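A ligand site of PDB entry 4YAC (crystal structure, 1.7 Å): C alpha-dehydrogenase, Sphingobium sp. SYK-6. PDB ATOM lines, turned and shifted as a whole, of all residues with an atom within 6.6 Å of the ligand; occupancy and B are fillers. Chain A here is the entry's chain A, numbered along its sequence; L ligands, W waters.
OD2 of Asp 38 is in hydrogen-bond range of O5 of the ligand (2.6 Å).
An oxygen (O10) of the ligand sits at hydrogen-bond distance from the backbone NH (N) of Val 18 (2.9 Å).
A ring nitrogen (ND1) of His 43 is in hydrogen-bond range of an oxygen (O5) of the ligand (2.9 Å).
The side-chain hydroxyl (OG) of Ser 16 lies within hydrogen-bond range of an oxygen (O2) of the ligand, at 3.0 Å.
N3 of the ligand sits at hydrogen-bond distance from OD1 of Asp 64 (3.1 Å).
The backbone NH of Leu 65 sits at hydrogen-bond distance from a nitrogen (N4) of the ligand (3.1 Å).
The backbone NH of Ile 39 is in hydrogen-bond range of a nitrogen (N5) of the ligand.
Water W3 lies within hydrogen-bond range of an oxygen (O10) of the ligand (2.5 Å), the backbone carbonyl oxygen of Ser 16 (2.9 Å) and the backbone NH of Ala 19 (3.1 Å).
Water W2 lies within hydrogen-bond range of O of Gly 93 (2.8 Å) and O7 of the ligand (3.3 Å).
The backbone NH (N) of Leu 63 is in hydrogen-bond range of the backbone carbonyl oxygen (O) of Asp 38, 2.8 Å away.
The backbone NH of Arg 40 lies within hydrogen-bond range of the side-chain carboxylate of Asp 38.
OD2 of Asp 38 sits at hydrogen-bond distance from N of Gly 15 (3.0 Å).
A ring nitrogen (NE2) of His 43 lies close to the guanidinium group of Arg 40 (3.2 Å).
The backbone NH of Ile 39 sits at hydrogen-bond distance from the backbone carbonyl oxygen of Leu 63 (3.1 Å).
The side-chain carboxylate of Asp 64 sits at hydrogen-bond distance from the side-chain hydroxyl of Thr 66 (2.8 Å).
The backbone carbonyl oxygen of Ala 37 sits at hydrogen-bond distance from the backbone NH of Gly 13, 2.7 Å away.
The backbone carbonyl oxygen (O) of Leu 63 sits close to a nitrogen (N4) of the ligand (3.4 Å).
Gly 13 touches the ligand (CA to O4, 3.5 Å).
CA of Gly 17 touches O10 of the ligand, at 3.4 Å.
CG of Arg 40 touches O6 of the ligand, at 3.8 Å.
CG1 of Val 94 touches C6 of the ligand, at 3.9 Å.
Val 114 touches the ligand.
Of the 26 residues printed, 13 come within 4 Å of the ligand.
Along chain A the residues within 4 Å of the ligand span positions 13 to 114.
The nearest printed residue that does not touch the ligand is Thr 66 (4.1 Å).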
ATOM      1  N   THR A  12      13.843 -20.903  -7.357  1.00  0.00           N
ATOM      2  CA  THR A  12      14.880 -19.926  -7.653  1.00  0.00           C
ATOM      3  C   THR A  12      15.151 -19.045  -6.437  1.00  0.00           C
ATOM      4  O   THR A  12      14.235 -18.719  -5.662  1.00  0.00           O
ATOM      5  CB  THR A  12      14.504 -19.041  -8.853  1.00  0.00           C
ATOM      6  OG1 THR A  12      13.446 -18.138  -8.494  1.00  0.00           O
ATOM      7  CG2 THR A  12      14.063 -19.898 -10.036  1.00  0.00           C
ATOM      8  N   GLY A  13      16.416 -18.682  -6.260  1.00  0.00           N
ATOM      9  CA  GLY A  13      16.841 -17.938  -5.093  1.00  0.00           C
ATOM     10  C   GLY A  13      16.857 -18.799  -3.852  1.00  0.00           C
ATOM     11  O   GLY A  13      16.963 -18.288  -2.740  1.00  0.00           O
ATOM     12  N   GLY A  14      16.798 -20.115  -4.035  1.00  0.00           N
ATOM     13  CA  GLY A  14      16.583 -21.066  -2.948  1.00  0.00           C
ATOM     14  C   GLY A  14      17.692 -21.196  -1.929  1.00  0.00           C
ATOM     15  O   GLY A  14      17.570 -21.958  -0.978  1.00  0.00           O
ATOM     16  N   GLY A  15      18.784 -20.460  -2.120  1.00  0.00           N
ATOM     17  CA  GLY A  15      19.909 -20.502  -1.194  1.00  0.00           C
ATOM     18  C   GLY A  15      19.719 -19.636   0.036  1.00  0.00           C
ATOM     19  O   GLY A  15      20.489 -19.747   0.995  1.00  0.00           O
ATOM     20  N   SER A  16      18.709 -18.766   0.027  1.00  0.00           N
ATOM     21  CA  SER A  16      18.526 -17.819   1.114  1.00  0.00           C
ATOM     22  C   SER A  16      17.097 -17.285   1.224  1.00  0.00           C
ATOM     23  O   SER A  16      16.303 -17.431   0.299  1.00  0.00           O
ATOM     24  CB  SER A  16      19.479 -16.629   0.937  1.00  0.00           C
ATOM     25  OG  SER A  16      19.452 -15.758   2.048  1.00  0.00           O
ATOM     26  N   GLY A  17      16.784 -16.697   2.368  1.00  0.00           N
ATOM     27  CA  GLY A  17      15.587 -15.894   2.536  1.00  0.00           C
ATOM     28  C   GLY A  17      14.269 -16.592   2.253  1.00  0.00           C
ATOM     29  O   GLY A  17      14.083 -17.757   2.603  1.00  0.00           O
ATOM     30  N   VAL A  18      13.359 -15.864   1.619  1.00  0.00           N
ATOM     31  CA  VAL A  18      12.010 -16.369   1.330  1.00  0.00           C
ATOM     32  C   VAL A  18      12.049 -17.662   0.540  1.00  0.00           C
ATOM     33  O   VAL A  18      11.314 -18.611   0.859  1.00  0.00           O
ATOM     34  CB  VAL A  18      11.180 -15.321   0.552  1.00  0.00           C
ATOM     35  CG1 VAL A  18       9.883 -15.924   0.014  1.00  0.00           C
ATOM     36  CG2 VAL A  18      10.874 -14.132   1.442  1.00  0.00           C
ATOM     37  N   ALA A  19      12.885 -17.715  -0.486  1.00  0.00           N
ATOM     38  CA  ALA A  19      12.930 -18.898  -1.351  1.00  0.00           C
ATOM     39  C   ALA A  19      13.432 -20.126  -0.606  1.00  0.00           C
ATOM     40  O   ALA A  19      12.934 -21.229  -0.806  1.00  0.00           O
ATOM     41  CB  ALA A  19      13.797 -18.623  -2.554  1.00  0.00           C
ATOM     42  N   LEU A  20      14.430 -19.948   0.257  1.00  0.00           N
ATOM     43  CA  LEU A  20      14.926 -21.043   1.075  1.00  0.00           C
ATOM     44  C   LEU A  20      13.816 -21.558   1.983  1.00  0.00           C
ATOM     45  O   LEU A  20      13.682 -22.766   2.188  1.00  0.00           O
ATOM     46  CB  LEU A  20      16.137 -20.608   1.907  1.00  0.00           C
ATOM     47  CG  LEU A  20      16.672 -21.618   2.926  1.00  0.00           C
ATOM     48  CD1 LEU A  20      17.006 -22.938   2.267  1.00  0.00           C
ATOM     49  CD2 LEU A  20      17.892 -21.059   3.630  1.00  0.00           C
ATOM     50  N   ALA A  37      17.979 -23.362  -6.914  1.00  0.00           N
ATOM     51  CA  ALA A  37      18.779 -22.692  -7.920  1.00  0.00           C
ATOM     52  C   ALA A  37      19.134 -21.300  -7.440  1.00  0.00           C
ATOM     53  O   ALA A  37      18.243 -20.514  -7.132  1.00  0.00           O
ATOM     54  CB  ALA A  37      18.036 -22.632  -9.236  1.00  0.00           C
ATOM     55  N   ASP A  38      20.429 -21.005  -7.374  1.00  0.00           N
ATOM     56  CA  ASP A  38      20.895 -19.758  -6.801  1.00  0.00           C
ATOM     57  C   ASP A  38      22.195 -19.321  -7.472  1.00  0.00           C
ATOM     58  O   ASP A  38      22.987 -20.156  -7.876  1.00  0.00           O
ATOM     59  CB  ASP A  38      21.108 -19.916  -5.300  1.00  0.00           C
ATOM     60  CG  ASP A  38      21.021 -18.606  -4.554  1.00  0.00           C
ATOM     61  OD1 ASP A  38      22.001 -17.832  -4.582  1.00  0.00           O
ATOM     62  OD2 ASP A  38      19.975 -18.365  -3.932  1.00  0.00           O
ATOM     63  N   ILE A  39      22.402 -18.015  -7.598  1.00  0.00           N
ATOM     64  CA  ILE A  39      23.615 -17.518  -8.228  1.00  0.00           C
ATOM     65  C   ILE A  39      24.816 -17.633  -7.290  1.00  0.00           C
ATOM     66  O   ILE A  39      25.942 -17.797  -7.760  1.00  0.00           O
ATOM     67  CB  ILE A  39      23.447 -16.055  -8.677  1.00  0.00           C
ATOM     68  CG1 ILE A  39      24.533 -15.684  -9.686  1.00  0.00           C
ATOM     69  CG2 ILE A  39      23.451 -15.101  -7.476  1.00  0.00           C
ATOM     70  CD1 ILE A  39      24.306 -14.320 -10.364  1.00  0.00           C
ATOM     71  N   ARG A  40      24.584 -17.584  -5.989  1.00  0.00           N
ATOM     72  CA  ARG A  40      25.679 -17.609  -5.025  1.00  0.00           C
ATOM     73  C   ARG A  40      25.999 -19.001  -4.513  1.00  0.00           C
ATOM     74  O   ARG A  40      25.159 -19.660  -3.893  1.00  0.00           O
ATOM     75  CB  ARG A  40      25.361 -16.691  -3.835  1.00  0.00           C
ATOM     76  CG  ARG A  40      25.630 -15.233  -4.153  1.00  0.00           C
ATOM     77  CD  ARG A  40      25.411 -14.338  -2.948  1.00  0.00           C
ATOM     78  NE  ARG A  40      26.330 -14.641  -1.859  1.00  0.00           N
ATOM     79  CZ  ARG A  40      26.426 -13.907  -0.747  1.00  0.00           C
ATOM     80  NH1 ARG A  40      25.672 -12.835  -0.587  1.00  0.00           N
ATOM     81  NH2 ARG A  40      27.296 -14.247   0.196  1.00  0.00           N
ATOM     82  N   HIS A  43      25.734 -19.466  -0.647  1.00  0.00           N
ATOM     83  CA  HIS A  43      24.371 -19.630  -0.146  1.00  0.00           C
ATOM     84  C   HIS A  43      23.886 -21.067  -0.340  1.00  0.00           C
ATOM     85  O   HIS A  43      23.264 -21.641   0.545  1.00  0.00           O
ATOM     86  CB  HIS A  43      23.415 -18.644  -0.837  1.00  0.00           C
ATOM     87  CG  HIS A  43      23.571 -17.233  -0.363  1.00  0.00           C
ATOM     88  ND1 HIS A  43      22.834 -16.196  -0.894  1.00  0.00           N
ATOM     89  CD2 HIS A  43      24.373 -16.689   0.588  1.00  0.00           C
ATOM     90  CE1 HIS A  43      23.183 -15.060  -0.287  1.00  0.00           C
ATOM     91  NE2 HIS A  43      24.107 -15.338   0.608  1.00  0.00           N
ATOM     92  N   LEU A  63      23.132 -21.083 -10.521  1.00  0.00           N
ATOM     93  CA  LEU A  63      22.499 -20.537 -11.720  1.00  0.00           C
ATOM     94  C   LEU A  63      22.238 -19.040 -11.589  1.00  0.00           C
ATOM     95  O   LEU A  63      21.662 -18.602 -10.601  1.00  0.00           O
ATOM     96  CB  LEU A  63      21.180 -21.255 -12.000  1.00  0.00           C
ATOM     97  CG  LEU A  63      20.277 -20.627 -13.064  1.00  0.00           C
ATOM     98  CD1 LEU A  63      20.931 -20.688 -14.436  1.00  0.00           C
ATOM     99  CD2 LEU A  63      18.922 -21.306 -13.077  1.00  0.00           C
ATOM    100  N   ASP A  64      22.691 -18.292 -12.592  1.00  0.00           N
ATOM    101  CA  ASP A  64      22.272 -16.916 -12.811  1.00  0.00           C
ATOM    102  C   ASP A  64      21.012 -16.939 -13.681  1.00  0.00           C
ATOM    103  O   ASP A  64      21.076 -17.306 -14.851  1.00  0.00           O
ATOM    104  CB  ASP A  64      23.391 -16.106 -13.487  1.00  0.00           C
ATOM    105  CG  ASP A  64      23.036 -14.637 -13.667  1.00  0.00           C
ATOM    106  OD1 ASP A  64      21.867 -14.253 -13.451  1.00  0.00           O
ATOM    107  OD2 ASP A  64      23.936 -13.860 -14.070  1.00  0.00           O
ATOM    108  N   LEU A  65      19.883 -16.568 -13.098  1.00  0.00           N
ATOM    109  CA  LEU A  65      18.584 -16.675 -13.776  1.00  0.00           C
ATOM    110  C   LEU A  65      18.489 -15.787 -15.001  1.00  0.00           C
ATOM    111  O   LEU A  65      17.610 -15.999 -15.847  1.00  0.00           O
ATOM    112  CB  LEU A  65      17.463 -16.331 -12.805  1.00  0.00           C
ATOM    113  CG  LEU A  65      17.440 -17.143 -11.512  1.00  0.00           C
ATOM    114  CD1 LEU A  65      16.554 -16.470 -10.482  1.00  0.00           C
ATOM    115  CD2 LEU A  65      16.987 -18.571 -11.778  1.00  0.00           C
ATOM    116  N   THR A  66      19.371 -14.795 -15.101  1.00  0.00           N
ATOM    117  CA  THR A  66      19.364 -13.891 -16.246  1.00  0.00           C
ATOM    118  C   THR A  66      20.077 -14.518 -17.448  1.00  0.00           C
ATOM    119  O   THR A  66      20.043 -13.961 -18.556  1.00  0.00           O
ATOM    120  CB  THR A  66      20.032 -12.535 -15.906  1.00  0.00           C
ATOM    121  OG1 THR A  66      21.441 -12.706 -15.733  1.00  0.00           O
ATOM    122  CG2 THR A  66      19.426 -11.945 -14.636  1.00  0.00           C
ATOM    123  N   THR A  91      11.011 -17.136  -7.348  1.00  0.00           N
ATOM    124  CA  THR A  91      11.013 -16.397  -6.088  1.00  0.00           C
ATOM    125  C   THR A  91      12.234 -15.497  -5.915  1.00  0.00           C
ATOM    126  O   THR A  91      12.180 -14.531  -5.162  1.00  0.00           O
ATOM    127  CB  THR A  91      10.904 -17.392  -4.912  1.00  0.00           C
ATOM    128  OG1 THR A  91       9.690 -18.138  -5.065  1.00  0.00           O
ATOM    129  CG2 THR A  91      10.882 -16.690  -3.566  1.00  0.00           C
ATOM    130  N   ALA A  92      13.320 -15.792  -6.621  1.00  0.00           N
ATOM    131  CA  ALA A  92      14.501 -14.936  -6.564  1.00  0.00           C
ATOM    132  C   ALA A  92      14.119 -13.505  -6.891  1.00  0.00           C
ATOM    133  O   ALA A  92      13.293 -13.248  -7.761  1.00  0.00           O
ATOM    134  CB  ALA A  92      15.575 -15.425  -7.515  1.00  0.00           C
ATOM    135  N   GLY A  93      14.716 -12.558  -6.172  1.00  0.00           N
ATOM    136  CA  GLY A  93      14.491 -11.160  -6.451  1.00  0.00           C
ATOM    137  C   GLY A  93      15.524 -10.317  -5.740  1.00  0.00           C
ATOM    138  O   GLY A  93      16.109 -10.737  -4.751  1.00  0.00           O
ATOM    139  N   VAL A  94      15.747  -9.107  -6.267  1.00  0.00           N
ATOM    140  CA  VAL A  94      16.668  -8.161  -5.652  1.00  0.00           C
ATOM    141  C   VAL A  94      15.988  -6.812  -5.509  1.00  0.00           C
ATOM    142  O   VAL A  94      14.934  -6.566  -6.099  1.00  0.00           O
ATOM    143  CB  VAL A  94      17.950  -7.979  -6.490  1.00  0.00           C
ATOM    144  CG1 VAL A  94      18.671  -9.310  -6.635  1.00  0.00           C
ATOM    145  CG2 VAL A  94      17.624  -7.404  -7.869  1.00  0.00           C
ATOM    146  N   TRP A 110      19.838  -3.944 -13.706  1.00  0.00           N
ATOM    147  CA  TRP A 110      20.071  -5.027 -12.744  1.00  0.00           C
ATOM    148  C   TRP A 110      18.759  -5.546 -12.163  1.00  0.00           C
ATOM    149  O   TRP A 110      18.492  -6.742 -12.215  1.00  0.00           O
ATOM    150  CB  TRP A 110      20.996  -4.537 -11.622  1.00  0.00           C
ATOM    151  CG  TRP A 110      21.100  -5.484 -10.459  1.00  0.00           C
ATOM    152  CD1 TRP A 110      21.307  -6.836 -10.510  1.00  0.00           C
ATOM    153  CD2 TRP A 110      21.010  -5.138  -9.075  1.00  0.00           C
ATOM    154  NE1 TRP A 110      21.348  -7.352  -9.247  1.00  0.00           N
ATOM    155  CE2 TRP A 110      21.174  -6.329  -8.342  1.00  0.00           C
ATOM    156  CE3 TRP A 110      20.809  -3.951  -8.385  1.00  0.00           C
ATOM    157  CZ2 TRP A 110      21.136  -6.359  -6.955  1.00  0.00           C
ATOM    158  CZ3 TRP A 110      20.781  -3.982  -7.008  1.00  0.00           C
ATOM    159  CH2 TRP A 110      20.945  -5.178  -6.304  1.00  0.00           C
ATOM    160  N   ASP A 113      16.472  -7.081 -14.853  1.00  0.00           N
ATOM    161  CA  ASP A 113      16.955  -8.360 -15.373  1.00  0.00           C
ATOM    162  C   ASP A 113      16.624  -9.503 -14.404  1.00  0.00           C
ATOM    163  O   ASP A 113      16.124 -10.546 -14.824  1.00  0.00           O
ATOM    164  CB  ASP A 113      18.467  -8.294 -15.645  1.00  0.00           C
ATOM    165  CG  ASP A 113      18.912  -9.238 -16.758  1.00  0.00           C
ATOM    166  OD1 ASP A 113      18.052  -9.807 -17.474  1.00  0.00           O
ATOM    167  OD2 ASP A 113      20.130  -9.406 -16.933  1.00  0.00           O
ATOM    168  N   VAL A 114      16.899  -9.321 -13.121  1.00  0.00           N
ATOM    169  CA  VAL A 114      16.631 -10.398 -12.159  1.00  0.00           C
ATOM    170  C   VAL A 114      15.145 -10.533 -11.867  1.00  0.00           C
ATOM    171  O   VAL A 114      14.602 -11.643 -11.916  1.00  0.00           O
ATOM    172  CB  VAL A 114      17.358 -10.170 -10.813  1.00  0.00           C
ATOM    173  CG1 VAL A 114      17.057 -11.303  -9.834  1.00  0.00           C
ATOM    174  CG2 VAL A 114      18.851 -10.066 -11.040  1.00  0.00           C
ATOM    175  N   PHE A 229       7.058 -11.870  10.131  1.00  0.00           N
ATOM    176  CA  PHE A 229       7.379 -12.702   8.980  1.00  0.00           C
ATOM    177  C   PHE A 229       8.430 -13.761   9.319  1.00  0.00           C
ATOM    178  O   PHE A 229       9.493 -13.440   9.851  1.00  0.00           O
ATOM    179  CB  PHE A 229       7.891 -11.857   7.823  1.00  0.00           C
ATOM    180  CG  PHE A 229       8.691 -12.634   6.805  1.00  0.00           C
ATOM    181  CD1 PHE A 229      10.075 -12.594   6.817  1.00  0.00           C
ATOM    182  CD2 PHE A 229       8.047 -13.417   5.871  1.00  0.00           C
ATOM    183  CE1 PHE A 229      10.806 -13.315   5.891  1.00  0.00           C
ATOM    184  CE2 PHE A 229       8.778 -14.138   4.945  1.00  0.00           C
ATOM    185  CZ  PHE A 229      10.162 -14.097   4.957  1.00  0.00           C
HETATM  186  P1  LIG L   1      17.754 -12.850  -0.014  1.00  0.00           P
HETATM  187  O1  LIG L   1      19.011 -12.022  -0.205  1.00  0.00           O
HETATM  188  O2  LIG L   1      17.720 -13.398   1.425  1.00  0.00           O
HETATM  189  O3  LIG L   1      17.744 -14.040  -1.031  1.00  0.00           O
HETATM  190  C1  LIG L   1      17.852 -13.779  -2.397  1.00  0.00           C
HETATM  191  C2  LIG L   1      18.496 -14.915  -3.066  1.00  0.00           C
HETATM  192  O4  LIG L   1      18.302 -14.760  -4.515  1.00  0.00           O
HETATM  193  C3  LIG L   1      19.930 -14.954  -2.810  1.00  0.00           C
HETATM  194  O5  LIG L   1      20.337 -16.270  -2.448  1.00  0.00           O
HETATM  195  C4  LIG L   1      20.554 -14.529  -4.038  1.00  0.00           C
HETATM  196  O6  LIG L   1      21.862 -15.102  -4.185  1.00  0.00           O
HETATM  197  C5  LIG L   1      19.638 -14.976  -5.064  1.00  0.00           C
HETATM  198  N1  LIG L   1      19.814 -14.288  -6.317  1.00  0.00           N
HETATM  199  C6  LIG L   1      19.965 -12.953  -6.549  1.00  0.00           C
HETATM  200  N2  LIG L   1      20.111 -12.727  -7.860  1.00  0.00           N
HETATM  201  C7  LIG L   1      20.071 -13.919  -8.534  1.00  0.00           C
HETATM  202  C8  LIG L   1      20.166 -14.328  -9.859  1.00  0.00           C
HETATM  203  N3  LIG L   1      20.360 -13.393 -10.924  1.00  0.00           N
HETATM  204  N4  LIG L   1      20.070 -15.649 -10.163  1.00  0.00           N
HETATM  205  C9  LIG L   1      19.900 -16.579  -9.199  1.00  0.00           C
HETATM  206  N5  LIG L   1      19.793 -16.224  -7.907  1.00  0.00           N
HETATM  207  C10 LIG L   1      19.887 -14.916  -7.551  1.00  0.00           C
HETATM  208  O7  LIG L   1      16.501 -11.984  -0.290  1.00  0.00           O
HETATM  209  P2  LIG L   1      15.087 -12.280   0.400  1.00  0.00           P
HETATM  210  O8  LIG L   1      15.217 -12.080   1.910  1.00  0.00           O
HETATM  211  O9  LIG L   1      13.989 -11.284  -0.194  1.00  0.00           O
HETATM  212  O10 LIG L   1      14.663 -13.742   0.120  1.00  0.00           O
HETATM  213  O   HOH W   1      21.815 -12.256  -0.632  1.00  0.00           O
HETATM  214  O   HOH W   2      17.495  -9.849  -2.545  1.00  0.00           O
HETATM  215  O   HOH W   3      14.956 -15.645  -1.550  1.00  0.00           O
HETATM  216  O   HOH W   4      18.952  -9.343   0.877  1.00  0.00           O
